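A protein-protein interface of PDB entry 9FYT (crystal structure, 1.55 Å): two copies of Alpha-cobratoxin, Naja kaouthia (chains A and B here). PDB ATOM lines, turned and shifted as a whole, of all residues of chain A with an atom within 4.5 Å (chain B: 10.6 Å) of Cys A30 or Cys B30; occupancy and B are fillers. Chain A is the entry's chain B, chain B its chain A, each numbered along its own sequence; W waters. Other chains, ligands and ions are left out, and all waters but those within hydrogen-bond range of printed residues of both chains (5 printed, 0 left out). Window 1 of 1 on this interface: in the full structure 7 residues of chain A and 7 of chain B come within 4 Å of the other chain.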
ATOM      1  N   CYS A  26      11.940  24.032 -13.207  1.00  0.00           N
ATOM      2  CA  CYS A  26      12.478  23.561 -11.934  1.00  0.00           C
ATOM      3  C   CYS A  26      11.811  22.255 -11.510  1.00  0.00           C
ATOM      4  O   CYS A  26      10.579  22.151 -11.520  1.00  0.00           O
ATOM      5  CB  CYS A  26      12.276  24.623 -10.852  1.00  0.00           C
ATOM      6  SG  CYS A  26      13.553  25.863 -10.685  1.00  0.00           S
ATOM      7  N   ASP A  27      12.625  21.255 -11.137  1.00  0.00           N
ATOM      8  CA  ASP A  27      12.101  20.103 -10.419  1.00  0.00           C
ATOM      9  C   ASP A  27      12.464  20.266  -8.937  1.00  0.00           C
ATOM     10  O   ASP A  27      12.886  21.335  -8.500  1.00  0.00           O
ATOM     11  CB  ASP A  27      12.583  18.777 -11.028  1.00  0.00           C
ATOM     12  CG  ASP A  27      14.043  18.442 -10.727  1.00  0.00           C
ATOM     13  OD1 ASP A  27      14.753  19.197 -10.037  1.00  0.00           O
ATOM     14  OD2 ASP A  27      14.494  17.383 -11.226  1.00  0.00           O
ATOM     15  N   ALA A  28      12.299  19.207  -8.149  1.00  0.00           N
ATOM     16  CA  ALA A  28      12.493  19.366  -6.713  1.00  0.00           C
ATOM     17  C   ALA A  28      13.948  19.604  -6.312  1.00  0.00           C
ATOM     18  O   ALA A  28      14.201  19.925  -5.129  1.00  0.00           O
ATOM     19  CB  ALA A  28      11.957  18.142  -5.956  1.00  0.00           C
ATOM     20  N   PHE A  29      14.900  19.422  -7.236  1.00  0.00           N
ATOM     21  CA  PHE A  29      16.321  19.630  -6.978  1.00  0.00           C
ATOM     22  C   PHE A  29      16.850  20.899  -7.636  1.00  0.00           C
ATOM     23  O   PHE A  29      18.067  21.073  -7.778  1.00  0.00           O
ATOM     24  CB  PHE A  29      17.103  18.398  -7.456  1.00  0.00           C
ATOM     25  CG  PHE A  29      16.701  17.147  -6.737  1.00  0.00           C
ATOM     26  CD1 PHE A  29      17.227  16.876  -5.491  1.00  0.00           C
ATOM     27  CD2 PHE A  29      15.782  16.279  -7.277  1.00  0.00           C
ATOM     28  CE1 PHE A  29      16.852  15.744  -4.807  1.00  0.00           C
ATOM     29  CE2 PHE A  29      15.411  15.144  -6.603  1.00  0.00           C
ATOM     30  CZ  PHE A  29      15.931  14.892  -5.360  1.00  0.00           C
ATOM     31  N   CYS A  30      15.949  21.811  -7.999  1.00  0.00           N
ATOM     32  CA  CYS A  30      16.344  23.009  -8.731  1.00  0.00           C
ATOM     33  C   CYS A  30      17.307  23.875  -7.946  1.00  0.00           C
ATOM     34  O   CYS A  30      18.160  24.531  -8.542  1.00  0.00           O
ATOM     35  CB  CYS A  30      15.094  23.790  -9.127  1.00  0.00           C
ATOM     36  SG  CYS A  30      15.378  24.891 -10.519  1.00  0.00           S
ATOM     37  N   SER A  31      17.192  23.921  -6.608  1.00  0.00           N
ATOM     38  CA  SER A  31      18.078  24.821  -5.884  1.00  0.00           C
ATOM     39  C   SER A  31      19.518  24.328  -5.928  1.00  0.00           C
ATOM     40  O   SER A  31      20.452  25.142  -6.008  1.00  0.00           O
ATOM     41  CB  SER A  31      17.621  24.986  -4.425  1.00  0.00           C
ATOM     42  OG  SER A  31      18.551  25.771  -3.680  1.00  0.00           O
ATOM     43  N   ILE A  32      19.732  23.003  -5.880  1.00  0.00           N
ATOM     44  CA  ILE A  32      21.098  22.507  -5.794  1.00  0.00           C
ATOM     45  C   ILE A  32      21.691  22.160  -7.168  1.00  0.00           C
ATOM     46  O   ILE A  32      22.907  22.229  -7.339  1.00  0.00           O
ATOM     47  CB  ILE A  32      21.203  21.289  -4.853  1.00  0.00           C
ATOM     48  CG1 ILE A  32      20.334  20.132  -5.320  1.00  0.00           C
ATOM     49  CG2 ILE A  32      20.848  21.685  -3.381  1.00  0.00           C
ATOM     50  CD1 ILE A  32      20.652  18.821  -4.592  1.00  0.00           C
ATOM     51  N   ARG A  33      20.866  21.781  -8.134  1.00  0.00           N
ATOM     52  CA  ARG A  33      21.325  21.353  -9.458  1.00  0.00           C
ATOM     53  C   ARG A  33      20.857  22.264 -10.583  1.00  0.00           C
ATOM     54  O   ARG A  33      21.116  21.973 -11.760  1.00  0.00           O
ATOM     55  CB  ARG A  33      20.825  19.928  -9.720  1.00  0.00           C
ATOM     56  CG  ARG A  33      21.566  18.840  -8.943  1.00  0.00           C
ATOM     57  CD  ARG A  33      22.882  18.498  -9.603  1.00  0.00           C
ATOM     58  NE  ARG A  33      23.566  17.392  -8.917  1.00  0.00           N
ATOM     59  CZ  ARG A  33      23.434  16.112  -9.238  1.00  0.00           C
ATOM     60  NH1 ARG A  33      22.588  15.719 -10.183  1.00  0.00           N
ATOM     61  NH2 ARG A  33      24.172  15.206  -8.598  1.00  0.00           N
ATOM     62  N   GLY A  34      20.176  23.340 -10.271  1.00  0.00           N
ATOM     63  CA  GLY A  34      19.712  24.243 -11.312  1.00  0.00           C
ATOM     64  C   GLY A  34      18.481  23.730 -12.026  1.00  0.00           C
ATOM     65  O   GLY A  34      17.965  22.634 -11.759  1.00  0.00           O
ATOM     66  N   LYS A  35      18.004  24.552 -12.962  1.00  0.00           N
ATOM     67  CA  LYS A  35      16.885  24.164 -13.797  1.00  0.00           C
ATOM     68  C   LYS A  35      17.264  22.953 -14.632  1.00  0.00           C
ATOM     69  O   LYS A  35      18.417  22.786 -15.019  1.00  0.00           O
ATOM     70  CB  LYS A  35      16.476  25.322 -14.733  1.00  0.00           C
ATOM     71  CG  LYS A  35      15.770  26.432 -13.970  1.00  0.00           C
ATOM     72  CD  LYS A  35      14.957  27.351 -14.854  1.00  0.00           C
ATOM     73  CE  LYS A  35      14.814  28.697 -14.204  1.00  0.00           C
ATOM     74  NZ  LYS A  35      13.949  29.616 -15.044  1.00  0.00           N
ATOM     75  N   ARG A  68      24.508  26.991 -15.077  1.00  0.00           N
ATOM     76  CA  ARG A  68      24.343  28.014 -14.061  1.00  0.00           C
ATOM     77  C   ARG A  68      25.710  28.592 -13.708  1.00  0.00           C
ATOM     78  O   ARG A  68      26.697  27.876 -13.593  1.00  0.00           O
ATOM     79  CB  ARG A  68      23.659  27.428 -12.823  1.00  0.00           C
ATOM     80  CG  ARG A  68      23.255  28.478 -11.828  1.00  0.00           C
ATOM     81  CD  ARG A  68      22.167  27.951 -10.855  1.00  0.00           C
ATOM     82  NE  ARG A  68      22.650  26.936  -9.935  1.00  0.00           N
ATOM     83  CZ  ARG A  68      21.939  26.451  -8.924  1.00  0.00           C
ATOM     84  NH1 ARG A  68      20.708  26.875  -8.669  1.00  0.00           N
ATOM     85  NH2 ARG A  68      22.476  25.519  -8.143  1.00  0.00           N
ATOM     86  N   LYS B  23       8.352  23.122   6.107  1.00  0.00           N
ATOM     87  CA  LYS B  23       7.953  22.569   4.816  1.00  0.00           C
ATOM     88  C   LYS B  23       8.741  23.286   3.730  1.00  0.00           C
ATOM     89  O   LYS B  23       8.760  24.518   3.717  1.00  0.00           O
ATOM     90  CB  LYS B  23       6.469  22.799   4.525  1.00  0.00           C
ATOM     91  CG  LYS B  23       5.448  22.021   5.303  1.00  0.00           C
ATOM     92  CD  LYS B  23       4.033  22.501   4.921  1.00  0.00           C
ATOM     93  CE  LYS B  23       2.957  21.922   5.847  1.00  0.00           C
ATOM     94  NZ  LYS B  23       1.660  22.644   5.758  1.00  0.00           N
ATOM     95  N   THR B  24       9.368  22.532   2.803  1.00  0.00           N
ATOM     96  CA  THR B  24      10.122  23.186   1.742  1.00  0.00           C
ATOM     97  C   THR B  24       9.838  22.543   0.391  1.00  0.00           C
ATOM     98  O   THR B  24       9.636  21.333   0.288  1.00  0.00           O
ATOM     99  CB  THR B  24      11.636  23.176   1.967  1.00  0.00           C
ATOM    100  OG1 THR B  24      12.123  21.832   2.041  1.00  0.00           O
ATOM    101  CG2 THR B  24      12.019  23.916   3.232  1.00  0.00           C
ATOM    102  N   TRP B  25       9.862  23.372  -0.653  1.00  0.00           N
ATOM    103  CA  TRP B  25       9.610  22.898  -2.005  1.00  0.00           C
ATOM    104  C   TRP B  25      10.138  23.930  -2.999  1.00  0.00           C
ATOM    105  O   TRP B  25      10.458  25.065  -2.626  1.00  0.00           O
ATOM    106  CB  TRP B  25       8.118  22.608  -2.244  1.00  0.00           C
ATOM    107  CG  TRP B  25       7.235  23.848  -2.312  1.00  0.00           C
ATOM    108  CD1 TRP B  25       6.793  24.490  -3.440  1.00  0.00           C
ATOM    109  CD2 TRP B  25       6.684  24.552  -1.203  1.00  0.00           C
ATOM    110  NE1 TRP B  25       6.008  25.589  -3.087  1.00  0.00           N
ATOM    111  CE2 TRP B  25       5.923  25.626  -1.715  1.00  0.00           C
ATOM    112  CE3 TRP B  25       6.752  24.377   0.187  1.00  0.00           C
ATOM    113  CZ2 TRP B  25       5.247  26.520  -0.878  1.00  0.00           C
ATOM    114  CZ3 TRP B  25       6.093  25.279   1.010  1.00  0.00           C
ATOM    115  CH2 TRP B  25       5.350  26.325   0.477  1.00  0.00           C
ATOM    116  N   CYS B  26      10.287  23.501  -4.258  1.00  0.00           N
ATOM    117  CA  CYS B  26      10.744  24.388  -5.325  1.00  0.00           C
ATOM    118  C   CYS B  26       9.557  24.925  -6.121  1.00  0.00           C
ATOM    119  O   CYS B  26       8.701  24.143  -6.571  1.00  0.00           O
ATOM    120  CB  CYS B  26      11.707  23.642  -6.261  1.00  0.00           C
ATOM    121  SG  CYS B  26      13.434  23.667  -5.762  1.00  0.00           S
ATOM    122  N   ASP B  27       9.504  26.254  -6.317  1.00  0.00           N
ATOM    123  CA  ASP B  27       8.651  26.818  -7.361  1.00  0.00           C
ATOM    124  C   ASP B  27       9.532  27.183  -8.567  1.00  0.00           C
ATOM    125  O   ASP B  27      10.695  26.770  -8.663  1.00  0.00           O
ATOM    126  CB  ASP B  27       7.815  27.985  -6.829  1.00  0.00           C
ATOM    127  CG  ASP B  27       8.598  29.259  -6.617  1.00  0.00           C
ATOM    128  OD1 ASP B  27       9.810  29.322  -6.897  1.00  0.00           O
ATOM    129  OD2 ASP B  27       7.952  30.246  -6.124  1.00  0.00           O
ATOM    130  N   ALA B  28       8.986  27.962  -9.507  1.00  0.00           N
ATOM    131  CA  ALA B  28       9.708  28.204 -10.755  1.00  0.00           C
ATOM    132  C   ALA B  28      10.953  29.055 -10.553  1.00  0.00           C
ATOM    133  O   ALA B  28      11.785  29.152 -11.466  1.00  0.00           O
ATOM    134  CB  ALA B  28       8.804  28.891 -11.778  1.00  0.00           C
ATOM    135  N   PHE B  29      11.072  29.728  -9.410  1.00  0.00           N
ATOM    136  CA  PHE B  29      12.206  30.590  -9.099  1.00  0.00           C
ATOM    137  C   PHE B  29      13.179  29.935  -8.122  1.00  0.00           C
ATOM    138  O   PHE B  29      14.041  30.620  -7.545  1.00  0.00           O
ATOM    139  CB  PHE B  29      11.679  31.913  -8.558  1.00  0.00           C
ATOM    140  CG  PHE B  29      10.861  32.656  -9.555  1.00  0.00           C
ATOM    141  CD1 PHE B  29      11.474  33.356 -10.579  1.00  0.00           C
ATOM    142  CD2 PHE B  29       9.486  32.627  -9.509  1.00  0.00           C
ATOM    143  CE1 PHE B  29      10.738  34.022 -11.501  1.00  0.00           C
ATOM    144  CE2 PHE B  29       8.741  33.337 -10.445  1.00  0.00           C
ATOM    145  CZ  PHE B  29       9.379  34.005 -11.448  1.00  0.00           C
ATOM    146  N   CYS B  30      13.086  28.616  -7.963  1.00  0.00           N
ATOM    147  CA  CYS B  30      13.899  27.920  -6.975  1.00  0.00           C
ATOM    148  C   CYS B  30      15.390  28.040  -7.254  1.00  0.00           C
ATOM    149  O   CYS B  30      16.200  28.021  -6.319  1.00  0.00           O
ATOM    150  CB  CYS B  30      13.488  26.456  -6.942  1.00  0.00           C
ATOM    151  SG  CYS B  30      13.949  25.651  -5.405  1.00  0.00           S
ATOM    152  N   SER B  31      15.788  28.141  -8.521  1.00  0.00           N
ATOM    153  CA  SER B  31      17.213  28.230  -8.783  1.00  0.00           C
ATOM    154  C   SER B  31      17.791  29.555  -8.292  1.00  0.00           C
ATOM    155  O   SER B  31      18.938  29.604  -7.813  1.00  0.00           O
ATOM    156  CB  SER B  31      17.500  28.029 -10.272  1.00  0.00           C
ATOM    157  OG  SER B  31      18.903  28.090 -10.500  1.00  0.00           O
ATOM    158  N   ILE B  32      17.031  30.646  -8.388  1.00  0.00           N
ATOM    159  CA  ILE B  32      17.628  31.943  -8.072  1.00  0.00           C
ATOM    160  C   ILE B  32      17.292  32.390  -6.650  1.00  0.00           C
ATOM    161  O   ILE B  32      18.078  33.109  -6.031  1.00  0.00           O
ATOM    162  CB  ILE B  32      17.223  33.042  -9.085  1.00  0.00           C
ATOM    163  CG1 ILE B  32      15.710  33.167  -9.203  1.00  0.00           C
ATOM    164  CG2 ILE B  32      17.875  32.751 -10.482  1.00  0.00           C
ATOM    165  CD1 ILE B  32      15.248  34.459  -9.900  1.00  0.00           C
ATOM    166  N   ARG B  33      16.148  31.961  -6.117  1.00  0.00           N
ATOM    167  CA  ARG B  33      15.696  32.376  -4.782  1.00  0.00           C
ATOM    168  C   ARG B  33      15.645  31.230  -3.763  1.00  0.00           C
ATOM    169  O   ARG B  33      15.167  31.419  -2.617  1.00  0.00           O
ATOM    170  CB  ARG B  33      14.317  33.028  -4.875  1.00  0.00           C
ATOM    171  CG  ARG B  33      14.297  34.423  -5.531  1.00  0.00           C
ATOM    172  CD  ARG B  33      14.608  35.508  -4.575  1.00  0.00           C
ATOM    173  NE  ARG B  33      14.499  36.853  -5.144  1.00  0.00           N
ATOM    174  CZ  ARG B  33      13.442  37.647  -5.025  1.00  0.00           C
ATOM    175  NH1 ARG B  33      12.329  37.224  -4.449  1.00  0.00           N
ATOM    176  NH2 ARG B  33      13.508  38.901  -5.498  1.00  0.00           N
ATOM    177  N   GLY B  34      16.130  30.057  -4.130  1.00  0.00           N
ATOM    178  CA  GLY B  34      16.107  28.925  -3.223  1.00  0.00           C
ATOM    179  C   GLY B  34      14.705  28.365  -3.080  1.00  0.00           C
ATOM    180  O   GLY B  34      13.737  28.825  -3.690  1.00  0.00           O
ATOM    181  N   LYS B  35      14.608  27.354  -2.215  1.00  0.00           N
ATOM    182  CA  LYS B  35      13.333  26.723  -1.943  1.00  0.00           C
ATOM    183  C   LYS B  35      12.410  27.694  -1.226  1.00  0.00           C
ATOM    184  O   LYS B  35      12.860  28.552  -0.470  1.00  0.00           O
ATOM    185  CB  LYS B  35      13.524  25.471  -1.076  1.00  0.00           C
ATOM    186  CG  LYS B  35      13.969  24.253  -1.912  1.00  0.00           C
ATOM    187  CD  LYS B  35      14.285  23.035  -1.088  1.00  0.00           C
ATOM    188  CE  LYS B  35      13.525  21.823  -1.591  1.00  0.00           C
ATOM    189  NZ  LYS B  35      13.397  20.720  -0.563  1.00  0.00           N
ATOM    190  N   ARG B  36      11.108  27.533  -1.455  1.00  0.00           N
ATOM    191  CA  ARG B  36      10.117  28.176  -0.603  1.00  0.00           C
ATOM    192  C   ARG B  36      10.079  27.432   0.722  1.00  0.00           C
ATOM    193  O   ARG B  36      10.166  26.196   0.738  1.00  0.00           O
ATOM    194  CB  ARG B  36       8.738  28.140  -1.235  1.00  0.00           C
ATOM    195  CG  ARG B  36       8.663  28.903  -2.559  1.00  0.00           C
ATOM    196  CD  ARG B  36       7.233  29.178  -2.933  1.00  0.00           C
ATOM    197  NE  ARG B  36       6.633  30.158  -2.028  1.00  0.00           N
ATOM    198  CZ  ARG B  36       6.731  31.469  -2.197  1.00  0.00           C
ATOM    199  NH1 ARG B  36       7.383  31.981  -3.227  1.00  0.00           N
ATOM    200  NH2 ARG B  36       6.189  32.283  -1.302  1.00  0.00           N
ATOM    201  N   VAL B  37       9.918  28.189   1.806  1.00  0.00           N
ATOM    202  CA  VAL B  37       9.920  27.675   3.164  1.00  0.00           C
ATOM    203  C   VAL B  37       8.631  28.094   3.866  1.00  0.00           C
ATOM    204  O   VAL B  37       8.304  29.287   3.920  1.00  0.00           O
ATOM    205  CB  VAL B  37      11.138  28.197   3.940  1.00  0.00           C
ATOM    206  CG1 VAL B  37      11.138  27.673   5.382  1.00  0.00           C
ATOM    207  CG2 VAL B  37      12.434  27.814   3.228  1.00  0.00           C
ATOM    208  N   GLY B  51       7.250  15.880  -3.860  1.00  0.00           N
ATOM    209  CA  GLY B  51       8.001  17.064  -4.203  1.00  0.00           C
ATOM    210  C   GLY B  51       8.177  18.049  -3.073  1.00  0.00           C
ATOM    211  O   GLY B  51       8.970  18.999  -3.203  1.00  0.00           O
ATOM    212  N   VAL B  52       7.464  17.859  -1.975  1.00  0.00           N
ATOM    213  CA  VAL B  52       7.541  18.729  -0.809  1.00  0.00           C
ATOM    214  C   VAL B  52       8.239  17.955   0.291  1.00  0.00           C
ATOM    215  O   VAL B  52       7.942  16.775   0.495  1.00  0.00           O
ATOM    216  CB  VAL B  52       6.145  19.183  -0.347  1.00  0.00           C
ATOM    217  CG1 VAL B  52       6.268  20.135   0.850  1.00  0.00           C
ATOM    218  CG2 VAL B  52       5.406  19.810  -1.525  1.00  0.00           C
ATOM    219  N   ARG B  68      19.645  29.729   2.363  1.00  0.00           N
ATOM    220  CA  ARG B  68      20.604  29.036   1.527  1.00  0.00           C
ATOM    221  C   ARG B  68      21.988  29.625   1.805  1.00  0.00           C
ATOM    222  O   ARG B  68      22.149  30.850   1.893  1.00  0.00           O
ATOM    223  CB  ARG B  68      20.214  29.175   0.048  1.00  0.00           C
ATOM    224  CG  ARG B  68      21.045  28.347  -0.894  1.00  0.00           C
ATOM    225  CD  ARG B  68      20.296  28.090  -2.212  1.00  0.00           C
ATOM    226  NE  ARG B  68      20.253  29.274  -3.050  1.00  0.00           N
ATOM    227  CZ  ARG B  68      19.824  29.287  -4.308  1.00  0.00           C
ATOM    228  NH1 ARG B  68      19.337  28.198  -4.891  1.00  0.00           N
ATOM    229  NH2 ARG B  68      19.879  30.426  -4.994  1.00  0.00           N
ATOM    230  N   LYS B  69      22.977  28.756   1.953  1.00  0.00           N
ATOM    231  CA  LYS B  69      24.358  29.193   2.082  1.00  0.00           C
ATOM    232  C   LYS B  69      24.851  29.709   0.741  1.00  0.00           C
ATOM    233  O   LYS B  69      24.708  29.027  -0.283  1.00  0.00           O
ATOM    234  CB  LYS B  69      25.248  28.043   2.542  1.00  0.00           C
ATOM    235  CG  LYS B  69      26.667  28.457   2.936  1.00  0.00           C
ATOM    236  CD  LYS B  69      27.426  27.235   3.480  1.00  0.00           C
ATOM    237  CE  LYS B  69      28.646  27.615   4.316  1.00  0.00           C
ATOM    238  NZ  LYS B  69      29.925  27.124   3.712  1.00  0.00           N
ATOM    239  N   ARG B  70      25.468  30.900   0.765  1.00  0.00           N
ATOM    240  CA  ARG B  70      25.863  31.629  -0.430  1.00  0.00           C
ATOM    241  C   ARG B  70      27.316  31.327  -0.741  1.00  0.00           C
ATOM    242  O   ARG B  70      28.198  31.786  -0.001  1.00  0.00           O
ATOM    243  CB  ARG B  70      25.669  33.133  -0.207  1.00  0.00           C
ATOM    244  CG  ARG B  70      24.217  33.561   0.002  1.00  0.00           C
ATOM    245  CD  ARG B  70      24.108  35.071   0.056  1.00  0.00           C
ATOM    246  NE  ARG B  70      24.539  35.670  -1.203  1.00  0.00           N
ATOM    247  CZ  ARG B  70      23.868  35.598  -2.344  1.00  0.00           C
ATOM    248  NH1 ARG B  70      22.683  35.010  -2.414  1.00  0.00           N
ATOM    249  NH2 ARG B  70      24.399  36.127  -3.445  1.00  0.00           N
HETATM  250  O   HOH W   1      17.236  26.658  -0.957  1.00  0.00           O
HETATM  251  O   HOH W   2      16.262  21.925  -4.618  1.00  0.00           O
HETATM  252  O   HOH W   3      12.019  31.053 -13.627  1.00  0.00           O
HETATM  253  O   HOH W   4      19.614  27.076 -13.450  1.00  0.00           O
HETATM  254  O   HOH W   5      14.652  29.430 -10.897  1.00  0.00           O
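Of the 20 printed residues of chain B, 6 touch a printed residue of chain A.
Of the 11 printed residues of chain A, 6 touch a printed residue of chain B.
Among the printed residues, no Asp or Glu carboxylate lies within 4 Å of a Lys or Arg side-chain nitrogen of the other chain.
Cys A26 touches Ala B28, and with the chains exchanged Ala A28 touches Cys B26.
Cys A26 touches Cys B30, and with the chains exchanged Cys A30 touches Cys B26.
Cys A30 touches Ser B31, and with the chains exchanged Ser A31 touches Cys B30.
Ser A31 touches Arg B68, and with the chains exchanged Arg A68 touches Ser B31.
Positions printed for both chains: 26, 27, 28, 29, 30, 31, 32, 33, 34, 35 and 68.
Of chain B, only Asp B27 (3.4 Å), Ala B28 (3.8 Å), Cys B30 (3.8 Å) and Ser B31 (3.9 Å) come within 4 Å of Cys A26.
Of chain B, only Cys B26 comes within 4 Å of Asp A27.
Ala A28 touches one residue of chain B.
Phe A29 touches none of the printed residues of chain B.
Cys A30 touches three residues of chain B.
Of the printed residues of chain B, Ser A31 touches Cys B26, Cys B30 and Arg B68.
No residue of chain B comes within 4 Å of Ile A32.
Printed residues of chain B within 4 Å of Arg A68: Ser B31 (2.8 Å).
Of the printed residues of chain A, Cys B26 touches Asp A27 (3.4 Å), Ala A28 (3.9 Å), Cys A30 (3.8 Å) and Ser A31 (3.9 Å).
Of the printed residues of chain A, Asp B27 touches Cys A26 (3.4 Å).
Cys B30 touches three residues of chain A.
The nearest printed residue of chain B that does not touch Cys A30 is Arg B68 (5.3 Å).
The nearest printed residue of chain A that does not touch Cys B30 is Arg A68 (5.2 Å).
N of Lys B35 lies within hydrogen-bond range of SG of Cys B30 (3.7 Å).
The side-chain sulfur (SG) of Cys A30 lies within hydrogen-bond range of the backbone NH (N) of Lys A35, 3.6 Å away.
NH2 of Arg A68 lies within hydrogen-bond range of O of Ser A31, at 3.0 Å.
SG of Cys B26 is disulfide-bonded to SG of Cys B30 (2.1 Å).
The guanidinium group (NH1) of Arg B68 sits at hydrogen-bond distance from the backbone carbonyl oxygen (O) of Cys B30 (3.5 Å).
SG of Cys A30 is disulfide-bonded to SG of Cys A26 (2.1 Å).
OG of Ser A31 lies within hydrogen-bond range of NH1 of Arg B68 (2.8 Å).
The side-chain sulfur (SG) of Cys B26 sits close to the backbone carbonyl oxygen (O) of Asp A27, at 3.6 Å.
SG of Cys A26 sits close to O of Asp B27 (3.6 Å).
The guanidinium group (NH1) of Arg A68 is in hydrogen-bond range of the side-chain hydroxyl (OG) of Ser B31, 2.8 Å away.
Cys A26 touches Ala B28 (SG to O, 3.8 Å).
Cys B30 touches Cys A26.
Ser B31 touches Cys A26.
O of Ala A28 touches SG of Cys B26 (3.9 Å).
CB of Cys A30 touches SG of Cys B26, at 3.8 Å.
CB of Cys A30 touches CB of Cys B30, 3.8 Å away.
SG of Cys A30 touches CB of Ser B31 (3.8 Å).
Cys B26 touches Ser A31 (SG to N, 3.9 Å).
Ser A31 touches Cys B30.
Water W3 bridges the side-chain amino group of Lys A35 and the backbone carbonyl oxygen of Ala B28.
Water W2 lies within hydrogen-bond range of the backbone carbonyl oxygen (O) of Ala A28 (2.9 Å), the backbone NH (N) of Ser A31 (3.0 Å), the backbone NH (N) of Cys A30 (3.4 Å) and the side-chain sulfur (SG) of Cys B26 (3.5 Å).
Water W5 lies within hydrogen-bond range of N of Ser B31, O of Ala B28, N of Cys B30 and SG of Cys A26.
Water W1 bridges N of Lys B35 (3.0 Å) and OG of Ser A31 (3.2 Å).
Water W4 bridges the backbone NH of Lys A35 (3.0 Å) and the side-chain hydroxyl of Ser B31 (3.2 Å).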
